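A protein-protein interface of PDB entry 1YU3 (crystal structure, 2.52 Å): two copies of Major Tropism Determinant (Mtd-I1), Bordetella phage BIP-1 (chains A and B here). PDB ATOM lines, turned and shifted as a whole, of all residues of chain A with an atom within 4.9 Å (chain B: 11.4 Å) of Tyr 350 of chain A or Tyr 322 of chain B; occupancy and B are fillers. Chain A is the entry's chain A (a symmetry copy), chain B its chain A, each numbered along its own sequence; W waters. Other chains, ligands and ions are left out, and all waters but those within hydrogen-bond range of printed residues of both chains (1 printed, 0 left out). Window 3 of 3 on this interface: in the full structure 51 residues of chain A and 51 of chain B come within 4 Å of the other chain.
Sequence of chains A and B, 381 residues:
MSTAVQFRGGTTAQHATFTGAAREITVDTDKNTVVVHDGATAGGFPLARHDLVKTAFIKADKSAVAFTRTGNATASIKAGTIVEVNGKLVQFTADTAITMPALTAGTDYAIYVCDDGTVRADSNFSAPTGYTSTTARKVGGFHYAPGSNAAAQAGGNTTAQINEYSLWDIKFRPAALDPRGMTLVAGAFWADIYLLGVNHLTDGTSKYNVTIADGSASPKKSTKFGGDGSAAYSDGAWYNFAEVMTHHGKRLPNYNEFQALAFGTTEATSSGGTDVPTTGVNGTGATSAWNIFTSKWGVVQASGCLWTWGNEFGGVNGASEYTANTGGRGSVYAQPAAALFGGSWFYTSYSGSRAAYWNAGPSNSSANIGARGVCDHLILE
Tyr 347 of chain A touches just one residue of chain B: Tyr 322.
No residue of chain B comes within 4 Å of Thr 348 of chain A.
No residue of chain B comes within 4 Å of Ser 349 of chain A.
Of chain B, only Tyr 322, Gly 330 and Ser 331 come within 4 Å of Tyr 350 of chain A.
Ser 351 of chain A touches just one residue of chain B: Gly 330.
Gly 352 of chain A touches just one residue of chain B: Arg 329 (3.4 Å).
Ala 355 of chain A touches two residues of chain B.
Of chain A, only Tyr 347, Tyr 350 and Tyr 357 come within 4 Å of Tyr 322 of chain B.
Of the printed residues of chain A, Arg 329 of chain B touches Gly 352 (3.4 Å) and Ala 355 (3.5 Å).
Of the printed residues of chain A, Gly 330 of chain B touches Tyr 350 (3.4 Å) and Ser 351 (3.6 Å).
The nearest residue of chain A that does not touch Tyr 322 of chain B is Trp 307 of chain A (4.5 Å).
The nearest printed residue of chain A that does not touch Arg 329 of chain B is Ser 351 of chain A (4.5 Å).
O of Ser 320 of chain B is in hydrogen-bond range of OH of Tyr 333 of chain B.
The side-chain hydroxyl of Thr 326 of chain B sits at hydrogen-bond distance from the backbone NH of Arg 329 of chain B, 3.1 Å away.
O of Gly 330 of chain B is in hydrogen-bond range of OG1 of Thr 326 of chain B, 2.7 Å away.
The side-chain hydroxyl (OG) of Ser 331 of chain B is in hydrogen-bond range of the backbone NH (N) of Ala 324 of chain B, at 3.4 Å.
Of the 20 printed residues of chain B, 5 touch a printed residue of chain A.
Hydrophobic or aromatic side chains of chain B within 4 Å of the printed part of chain A: Tyr 322 and Tyr 333.
Among the printed residues, no Asp or Glu carboxylate lies within 4 Å of a Lys or Arg side-chain nitrogen of the other chain.
CE2 of Tyr 347 of chain A touches OH of Tyr 322 of chain B (3.2 Å).
Tyr 322 of chain B touches Tyr 350 of chain A (CB to CD1, 3.7 Å).
Tyr 350 of chain A touches Gly 330 of chain B.
Gly 330 of chain B touches Ser 351 of chain A.
Arg 329 of chain B touches Gly 352 of chain A (O to C, 3.4 Å).
O of Arg 329 of chain B touches N of Ala 355 of chain A, 3.5 Å away.
Ser 331 of chain B touches Ala 355 of chain A.
Tyr 357 of chain A touches Tyr 322 of chain B (CD1 to OH, 3.4 Å).
CE1 of Tyr 357 of chain A touches CD2 of Tyr 333 of chain B, at 3.5 Å.
No position is printed for both chains.
Water W1 bridges the side-chain hydroxyl of Ser 331 of chain B (2.7 Å) and the backbone carbonyl oxygen of Ser 349 of chain A (2.8 Å).
The backbone carbonyl oxygen (O) of Tyr 350 of chain A is in hydrogen-bond range of the backbone NH (N) of Ser 331 of chain B (2.8 Å).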
ATOM      1  N   TRP A 307     -18.048   6.187 -19.528  1.00  0.00           N
ATOM      2  CA  TRP A 307     -17.931   5.401 -20.754  1.00  0.00           C
ATOM      3  C   TRP A 307     -18.573   6.196 -21.876  1.00  0.00           C
ATOM      4  O   TRP A 307     -19.546   6.914 -21.651  1.00  0.00           O
ATOM      5  CB  TRP A 307     -18.690   4.079 -20.640  1.00  0.00           C
ATOM      6  CG  TRP A 307     -18.139   3.063 -19.698  1.00  0.00           C
ATOM      7  CD1 TRP A 307     -18.583   2.802 -18.440  1.00  0.00           C
ATOM      8  CD2 TRP A 307     -17.081   2.129 -19.955  1.00  0.00           C
ATOM      9  NE1 TRP A 307     -17.858   1.778 -17.887  1.00  0.00           N
ATOM     10  CE2 TRP A 307     -16.928   1.346 -18.794  1.00  0.00           C
ATOM     11  CE3 TRP A 307     -16.241   1.884 -21.051  1.00  0.00           C
ATOM     12  CZ2 TRP A 307     -15.969   0.330 -18.693  1.00  0.00           C
ATOM     13  CZ3 TRP A 307     -15.281   0.870 -20.950  1.00  0.00           C
ATOM     14  CH2 TRP A 307     -15.158   0.108 -19.781  1.00  0.00           C
ATOM     15  N   TYR A 347     -14.313   2.556 -11.985  1.00  0.00           N
ATOM     16  CA  TYR A 347     -13.522   1.462 -12.581  1.00  0.00           C
ATOM     17  C   TYR A 347     -12.008   1.418 -12.350  1.00  0.00           C
ATOM     18  O   TYR A 347     -11.283   0.742 -13.088  1.00  0.00           O
ATOM     19  CB  TYR A 347     -13.885   1.291 -14.059  1.00  0.00           C
ATOM     20  CG  TYR A 347     -15.252   0.668 -14.205  1.00  0.00           C
ATOM     21  CD1 TYR A 347     -16.401   1.459 -14.184  1.00  0.00           C
ATOM     22  CD2 TYR A 347     -15.403  -0.718 -14.313  1.00  0.00           C
ATOM     23  CE1 TYR A 347     -17.667   0.894 -14.295  1.00  0.00           C
ATOM     24  CE2 TYR A 347     -16.668  -1.300 -14.422  1.00  0.00           C
ATOM     25  CZ  TYR A 347     -17.796  -0.486 -14.411  1.00  0.00           C
ATOM     26  OH  TYR A 347     -19.055  -1.043 -14.522  1.00  0.00           O
ATOM     27  N   THR A 348     -11.554   2.098 -11.298  1.00  0.00           N
ATOM     28  CA  THR A 348     -10.158   2.065 -10.837  1.00  0.00           C
ATOM     29  C   THR A 348      -9.125   1.963 -11.968  1.00  0.00           C
ATOM     30  O   THR A 348      -9.041   2.861 -12.809  1.00  0.00           O
ATOM     31  CB  THR A 348      -9.932   1.012  -9.675  1.00  0.00           C
ATOM     32  OG1 THR A 348      -8.564   1.027  -9.245  1.00  0.00           O
ATOM     33  CG2 THR A 348     -10.336  -0.411 -10.077  1.00  0.00           C
ATOM     34  N   SER A 349      -8.360   0.876 -11.995  1.00  0.00           N
ATOM     35  CA  SER A 349      -7.267   0.714 -12.943  1.00  0.00           C
ATOM     36  C   SER A 349      -7.710   0.194 -14.315  1.00  0.00           C
ATOM     37  O   SER A 349      -6.883   0.060 -15.225  1.00  0.00           O
ATOM     38  CB  SER A 349      -6.209  -0.222 -12.356  1.00  0.00           C
ATOM     39  OG  SER A 349      -6.752  -1.512 -12.134  1.00  0.00           O
ATOM     40  N   TYR A 350      -8.997  -0.107 -14.462  1.00  0.00           N
ATOM     41  CA  TYR A 350      -9.504  -0.662 -15.718  1.00  0.00           C
ATOM     42  C   TYR A 350      -9.654   0.406 -16.800  1.00  0.00           C
ATOM     43  O   TYR A 350      -9.612   0.093 -17.993  1.00  0.00           O
ATOM     44  CB  TYR A 350     -10.842  -1.377 -15.508  1.00  0.00           C
ATOM     45  CG  TYR A 350     -10.829  -2.428 -14.418  1.00  0.00           C
ATOM     46  CD1 TYR A 350      -9.764  -3.324 -14.296  1.00  0.00           C
ATOM     47  CD2 TYR A 350     -11.895  -2.543 -13.523  1.00  0.00           C
ATOM     48  CE1 TYR A 350      -9.751  -4.302 -13.298  1.00  0.00           C
ATOM     49  CE2 TYR A 350     -11.896  -3.520 -12.524  1.00  0.00           C
ATOM     50  CZ  TYR A 350     -10.818  -4.392 -12.416  1.00  0.00           C
ATOM     51  OH  TYR A 350     -10.793  -5.357 -11.434  1.00  0.00           O
ATOM     52  N   SER A 351      -9.825   1.659 -16.371  1.00  0.00           N
ATOM     53  CA  SER A 351     -10.000   2.802 -17.269  1.00  0.00           C
ATOM     54  C   SER A 351      -8.722   3.181 -18.022  1.00  0.00           C
ATOM     55  O   SER A 351      -7.606   2.906 -17.567  1.00  0.00           O
ATOM     56  CB  SER A 351     -10.507   4.013 -16.487  1.00  0.00           C
ATOM     57  OG  SER A 351     -11.778   3.766 -15.912  1.00  0.00           O
ATOM     58  N   GLY A 352      -8.897   3.819 -19.175  1.00  0.00           N
ATOM     59  CA  GLY A 352      -7.768   4.293 -19.965  1.00  0.00           C
ATOM     60  C   GLY A 352      -8.133   4.557 -21.412  1.00  0.00           C
ATOM     61  O   GLY A 352      -9.289   4.377 -21.814  1.00  0.00           O
ATOM     62  N   ALA A 355      -9.525   1.326 -22.757  1.00  0.00           N
ATOM     63  CA  ALA A 355     -10.571   0.637 -22.000  1.00  0.00           C
ATOM     64  C   ALA A 355     -11.758   0.390 -22.916  1.00  0.00           C
ATOM     65  O   ALA A 355     -12.277   1.328 -23.536  1.00  0.00           O
ATOM     66  CB  ALA A 355     -10.994   1.459 -20.797  1.00  0.00           C
ATOM     67  N   TYR A 357     -15.393  -2.193 -23.314  1.00  0.00           N
ATOM     68  CA  TYR A 357     -16.338  -3.154 -22.770  1.00  0.00           C
ATOM     69  C   TYR A 357     -17.325  -3.555 -23.863  1.00  0.00           C
ATOM     70  O   TYR A 357     -17.958  -2.693 -24.486  1.00  0.00           O
ATOM     71  CB  TYR A 357     -17.064  -2.535 -21.578  1.00  0.00           C
ATOM     72  CG  TYR A 357     -18.044  -3.426 -20.845  1.00  0.00           C
ATOM     73  CD1 TYR A 357     -17.641  -4.170 -19.734  1.00  0.00           C
ATOM     74  CD2 TYR A 357     -19.389  -3.480 -21.226  1.00  0.00           C
ATOM     75  CE1 TYR A 357     -18.540  -4.968 -19.038  1.00  0.00           C
ATOM     76  CE2 TYR A 357     -20.302  -4.278 -20.538  1.00  0.00           C
ATOM     77  CZ  TYR A 357     -19.865  -5.018 -19.447  1.00  0.00           C
ATOM     78  OH  TYR A 357     -20.755  -5.803 -18.759  1.00  0.00           O
ATOM     79  N   TYR B 239      -3.439  -2.429 -31.894  1.00  0.00           N
ATOM     80  CA  TYR B 239      -3.384  -1.109 -31.289  1.00  0.00           C
ATOM     81  C   TYR B 239      -2.284  -0.230 -31.885  1.00  0.00           C
ATOM     82  O   TYR B 239      -2.499   0.963 -32.138  1.00  0.00           O
ATOM     83  CB  TYR B 239      -3.189  -1.223 -29.789  1.00  0.00           C
ATOM     84  CG  TYR B 239      -4.328  -1.884 -29.050  1.00  0.00           C
ATOM     85  CD1 TYR B 239      -5.599  -1.293 -28.995  1.00  0.00           C
ATOM     86  CD2 TYR B 239      -4.130  -3.094 -28.375  1.00  0.00           C
ATOM     87  CE1 TYR B 239      -6.643  -1.904 -28.288  1.00  0.00           C
ATOM     88  CE2 TYR B 239      -5.163  -3.704 -27.669  1.00  0.00           C
ATOM     89  CZ  TYR B 239      -6.413  -3.113 -27.629  1.00  0.00           C
ATOM     90  OH  TYR B 239      -7.426  -3.738 -26.931  1.00  0.00           O
ATOM     91  N   GLY B 318     -12.381 -12.571 -26.446  1.00  0.00           N
ATOM     92  CA  GLY B 318     -11.583 -12.818 -25.251  1.00  0.00           C
ATOM     93  C   GLY B 318     -12.485 -13.043 -24.046  1.00  0.00           C
ATOM     94  O   GLY B 318     -13.713 -13.046 -24.164  1.00  0.00           O
ATOM     95  N   ALA B 319     -11.872 -13.226 -22.886  1.00  0.00           N
ATOM     96  CA  ALA B 319     -12.604 -13.544 -21.660  1.00  0.00           C
ATOM     97  C   ALA B 319     -13.594 -12.451 -21.275  1.00  0.00           C
ATOM     98  O   ALA B 319     -13.376 -11.269 -21.562  1.00  0.00           O
ATOM     99  CB  ALA B 319     -11.625 -13.789 -20.517  1.00  0.00           C
ATOM    100  N   SER B 320     -14.683 -12.853 -20.626  1.00  0.00           N
ATOM    101  CA  SER B 320     -15.601 -11.888 -20.032  1.00  0.00           C
ATOM    102  C   SER B 320     -15.105 -11.464 -18.649  1.00  0.00           C
ATOM    103  O   SER B 320     -15.794 -11.632 -17.641  1.00  0.00           O
ATOM    104  CB  SER B 320     -17.019 -12.445 -19.972  1.00  0.00           C
ATOM    105  OG  SER B 320     -17.495 -12.711 -21.278  1.00  0.00           O
ATOM    106  N   GLU B 321     -13.884 -10.938 -18.617  1.00  0.00           N
ATOM    107  CA  GLU B 321     -13.325 -10.313 -17.425  1.00  0.00           C
ATOM    108  C   GLU B 321     -12.402  -9.189 -17.854  1.00  0.00           C
ATOM    109  O   GLU B 321     -11.905  -9.185 -18.984  1.00  0.00           O
ATOM    110  CB  GLU B 321     -12.596 -11.327 -16.539  1.00  0.00           C
ATOM    111  CG  GLU B 321     -11.447 -12.078 -17.199  1.00  0.00           C
ATOM    112  CD  GLU B 321     -11.369 -13.526 -16.741  1.00  0.00           C
ATOM    113  OE1 GLU B 321     -12.056 -13.879 -15.751  1.00  0.00           O
ATOM    114  OE2 GLU B 321     -10.629 -14.311 -17.377  1.00  0.00           O
ATOM    115  N   TYR B 322     -12.175  -8.238 -16.955  1.00  0.00           N
ATOM    116  CA  TYR B 322     -11.346  -7.094 -17.280  1.00  0.00           C
ATOM    117  C   TYR B 322      -9.887  -7.504 -17.470  1.00  0.00           C
ATOM    118  O   TYR B 322      -9.187  -7.800 -16.507  1.00  0.00           O
ATOM    119  CB  TYR B 322     -11.523  -5.996 -16.229  1.00  0.00           C
ATOM    120  CG  TYR B 322     -12.891  -5.349 -16.312  1.00  0.00           C
ATOM    121  CD1 TYR B 322     -13.173  -4.388 -17.288  1.00  0.00           C
ATOM    122  CD2 TYR B 322     -13.911  -5.720 -15.436  1.00  0.00           C
ATOM    123  CE1 TYR B 322     -14.428  -3.800 -17.379  1.00  0.00           C
ATOM    124  CE2 TYR B 322     -15.171  -5.145 -15.518  1.00  0.00           C
ATOM    125  CZ  TYR B 322     -15.424  -4.186 -16.490  1.00  0.00           C
ATOM    126  OH  TYR B 322     -16.676  -3.614 -16.572  1.00  0.00           O
ATOM    127  N   THR B 323      -9.442  -7.539 -18.723  1.00  0.00           N
ATOM    128  CA  THR B 323      -8.092  -7.985 -19.039  1.00  0.00           C
ATOM    129  C   THR B 323      -7.213  -6.811 -19.459  1.00  0.00           C
ATOM    130  O   THR B 323      -7.483  -6.141 -20.455  1.00  0.00           O
ATOM    131  CB  THR B 323      -8.098  -9.074 -20.144  1.00  0.00           C
ATOM    132  OG1 THR B 323      -9.113 -10.046 -19.858  1.00  0.00           O
ATOM    133  CG2 THR B 323      -6.720  -9.761 -20.257  1.00  0.00           C
ATOM    134  N   ALA B 324      -6.154  -6.573 -18.691  1.00  0.00           N
ATOM    135  CA  ALA B 324      -5.219  -5.498 -18.985  1.00  0.00           C
ATOM    136  C   ALA B 324      -4.153  -5.964 -19.977  1.00  0.00           C
ATOM    137  O   ALA B 324      -3.035  -6.307 -19.594  1.00  0.00           O
ATOM    138  CB  ALA B 324      -4.582  -4.960 -17.695  1.00  0.00           C
ATOM    139  N   ASN B 325      -4.512  -5.964 -21.256  1.00  0.00           N
ATOM    140  CA  ASN B 325      -3.596  -6.383 -22.324  1.00  0.00           C
ATOM    141  C   ASN B 325      -3.464  -5.332 -23.431  1.00  0.00           C
ATOM    142  O   ASN B 325      -3.246  -5.671 -24.595  1.00  0.00           O
ATOM    143  CB  ASN B 325      -4.056  -7.724 -22.914  1.00  0.00           C
ATOM    144  CG  ASN B 325      -5.499  -7.682 -23.418  1.00  0.00           C
ATOM    145  OD1 ASN B 325      -6.135  -6.621 -23.462  1.00  0.00           O
ATOM    146  ND2 ASN B 325      -6.022  -8.839 -23.788  1.00  0.00           N
ATOM    147  N   THR B 326      -3.589  -4.060 -23.062  1.00  0.00           N
ATOM    148  CA  THR B 326      -3.643  -2.976 -24.040  1.00  0.00           C
ATOM    149  C   THR B 326      -2.346  -2.164 -24.097  1.00  0.00           C
ATOM    150  O   THR B 326      -2.319  -1.055 -24.645  1.00  0.00           O
ATOM    151  CB  THR B 326      -4.835  -2.019 -23.761  1.00  0.00           C
ATOM    152  OG1 THR B 326      -4.656  -1.380 -22.496  1.00  0.00           O
ATOM    153  CG2 THR B 326      -6.154  -2.775 -23.749  1.00  0.00           C
ATOM    154  N   GLY B 327      -1.272  -2.713 -23.537  1.00  0.00           N
ATOM    155  CA  GLY B 327      -0.020  -1.976 -23.431  1.00  0.00           C
ATOM    156  C   GLY B 327      -0.037  -0.983 -22.283  1.00  0.00           C
ATOM    157  O   GLY B 327       0.710  -0.012 -22.290  1.00  0.00           O
ATOM    158  N   GLY B 328      -0.896  -1.228 -21.295  1.00  0.00           N
ATOM    159  CA  GLY B 328      -0.977  -0.390 -20.093  1.00  0.00           C
ATOM    160  C   GLY B 328      -1.875   0.827 -20.243  1.00  0.00           C
ATOM    161  O   GLY B 328      -1.702   1.828 -19.540  1.00  0.00           O
ATOM    162  N   ARG B 329      -2.834   0.732 -21.163  1.00  0.00           N
ATOM    163  CA  ARG B 329      -3.766   1.828 -21.432  1.00  0.00           C
ATOM    164  C   ARG B 329      -5.218   1.423 -21.139  1.00  0.00           C
ATOM    165  O   ARG B 329      -6.160   1.865 -21.811  1.00  0.00           O
ATOM    166  CB  ARG B 329      -3.593   2.330 -22.867  1.00  0.00           C
ATOM    167  CG  ARG B 329      -2.193   2.860 -23.157  1.00  0.00           C
ATOM    168  CD  ARG B 329      -2.112   3.511 -24.515  1.00  0.00           C
ATOM    169  NE  ARG B 329      -0.726   3.784 -24.874  1.00  0.00           N
ATOM    170  CZ  ARG B 329      -0.320   4.270 -26.049  1.00  0.00           C
ATOM    171  NH1 ARG B 329      -1.193   4.565 -27.007  1.00  0.00           N
ATOM    172  NH2 ARG B 329       0.975   4.474 -26.259  1.00  0.00           N
ATOM    173  N   GLY B 330      -5.385   0.575 -20.126  1.00  0.00           N
ATOM    174  CA  GLY B 330      -6.706   0.146 -19.676  1.00  0.00           C
ATOM    175  C   GLY B 330      -6.983  -1.328 -19.882  1.00  0.00           C
ATOM    176  O   GLY B 330      -6.127  -2.079 -20.368  1.00  0.00           O
ATOM    177  N   SER B 331      -8.197  -1.734 -19.522  1.00  0.00           N
ATOM    178  CA  SER B 331      -8.613  -3.126 -19.606  1.00  0.00           C
ATOM    179  C   SER B 331      -9.749  -3.326 -20.598  1.00  0.00           C
ATOM    180  O   SER B 331     -10.539  -2.409 -20.849  1.00  0.00           O
ATOM    181  CB  SER B 331      -9.024  -3.642 -18.224  1.00  0.00           C
ATOM    182  OG  SER B 331      -7.884  -3.930 -17.436  1.00  0.00           O
ATOM    183  N   VAL B 332      -9.814  -4.531 -21.164  1.00  0.00           N
ATOM    184  CA  VAL B 332     -10.885  -4.905 -22.093  1.00  0.00           C
ATOM    185  C   VAL B 332     -11.729  -6.047 -21.534  1.00  0.00           C
ATOM    186  O   VAL B 332     -11.209  -6.960 -20.883  1.00  0.00           O
ATOM    187  CB  VAL B 332     -10.358  -5.276 -23.519  1.00  0.00           C
ATOM    188  CG1 VAL B 332      -9.678  -4.076 -24.165  1.00  0.00           C
ATOM    189  CG2 VAL B 332      -9.430  -6.481 -23.483  1.00  0.00           C
ATOM    190  N   TYR B 333     -13.030  -5.990 -21.798  1.00  0.00           N
ATOM    191  CA  TYR B 333     -13.964  -6.980 -21.285  1.00  0.00           C
ATOM    192  C   TYR B 333     -14.713  -7.587 -22.455  1.00  0.00           C
ATOM    193  O   TYR B 333     -15.359  -6.874 -23.215  1.00  0.00           O
ATOM    194  CB  TYR B 333     -14.938  -6.317 -20.319  1.00  0.00           C
ATOM    195  CG  TYR B 333     -15.833  -7.274 -19.569  1.00  0.00           C
ATOM    196  CD1 TYR B 333     -15.579  -7.592 -18.238  1.00  0.00           C
ATOM    197  CD2 TYR B 333     -16.939  -7.849 -20.184  1.00  0.00           C
ATOM    198  CE1 TYR B 333     -16.398  -8.457 -17.546  1.00  0.00           C
ATOM    199  CE2 TYR B 333     -17.760  -8.718 -19.504  1.00  0.00           C
ATOM    200  CZ  TYR B 333     -17.489  -9.023 -18.184  1.00  0.00           C
ATOM    201  OH  TYR B 333     -18.321  -9.895 -17.504  1.00  0.00           O
ATOM    202  N   ALA B 334     -14.617  -8.908 -22.586  1.00  0.00           N
ATOM    203  CA  ALA B 334     -15.199  -9.653 -23.708  1.00  0.00           C
ATOM    204  C   ALA B 334     -14.798  -9.058 -25.068  1.00  0.00           C
ATOM    205  O   ALA B 334     -15.637  -8.842 -25.942  1.00  0.00           O
ATOM    206  CB  ALA B 334     -16.723  -9.764 -23.561  1.00  0.00           C
ATOM    207  N   GLN B 335     -13.501  -8.812 -25.226  1.00  0.00           N
ATOM    208  CA  GLN B 335     -12.965  -8.163 -26.403  1.00  0.00           C
ATOM    209  C   GLN B 335     -13.060  -9.055 -27.642  1.00  0.00           C
ATOM    210  O   GLN B 335     -12.438 -10.109 -27.692  1.00  0.00           O
ATOM    211  CB  GLN B 335     -11.509  -7.774 -26.146  1.00  0.00           C
ATOM    212  CG  GLN B 335     -10.785  -7.214 -27.358  1.00  0.00           C
ATOM    213  CD  GLN B 335     -11.356  -5.887 -27.818  1.00  0.00           C
ATOM    214  OE1 GLN B 335     -11.518  -4.960 -27.022  1.00  0.00           O
ATOM    215  NE2 GLN B 335     -11.657  -5.785 -29.107  1.00  0.00           N
ATOM    216  N   SER B 363      -4.684  -7.466 -29.238  1.00  0.00           N
ATOM    217  CA  SER B 363      -3.413  -7.493 -28.517  1.00  0.00           C
ATOM    218  C   SER B 363      -2.436  -8.547 -29.051  1.00  0.00           C
ATOM    219  O   SER B 363      -1.318  -8.668 -28.550  1.00  0.00           O
ATOM    220  CB  SER B 363      -3.646  -7.698 -27.014  1.00  0.00           C
ATOM    221  OG  SER B 363      -4.286  -8.935 -26.752  1.00  0.00           O
HETATM  222  O   HOH W   1      -6.077  -2.063 -16.834  1.00  0.00           O
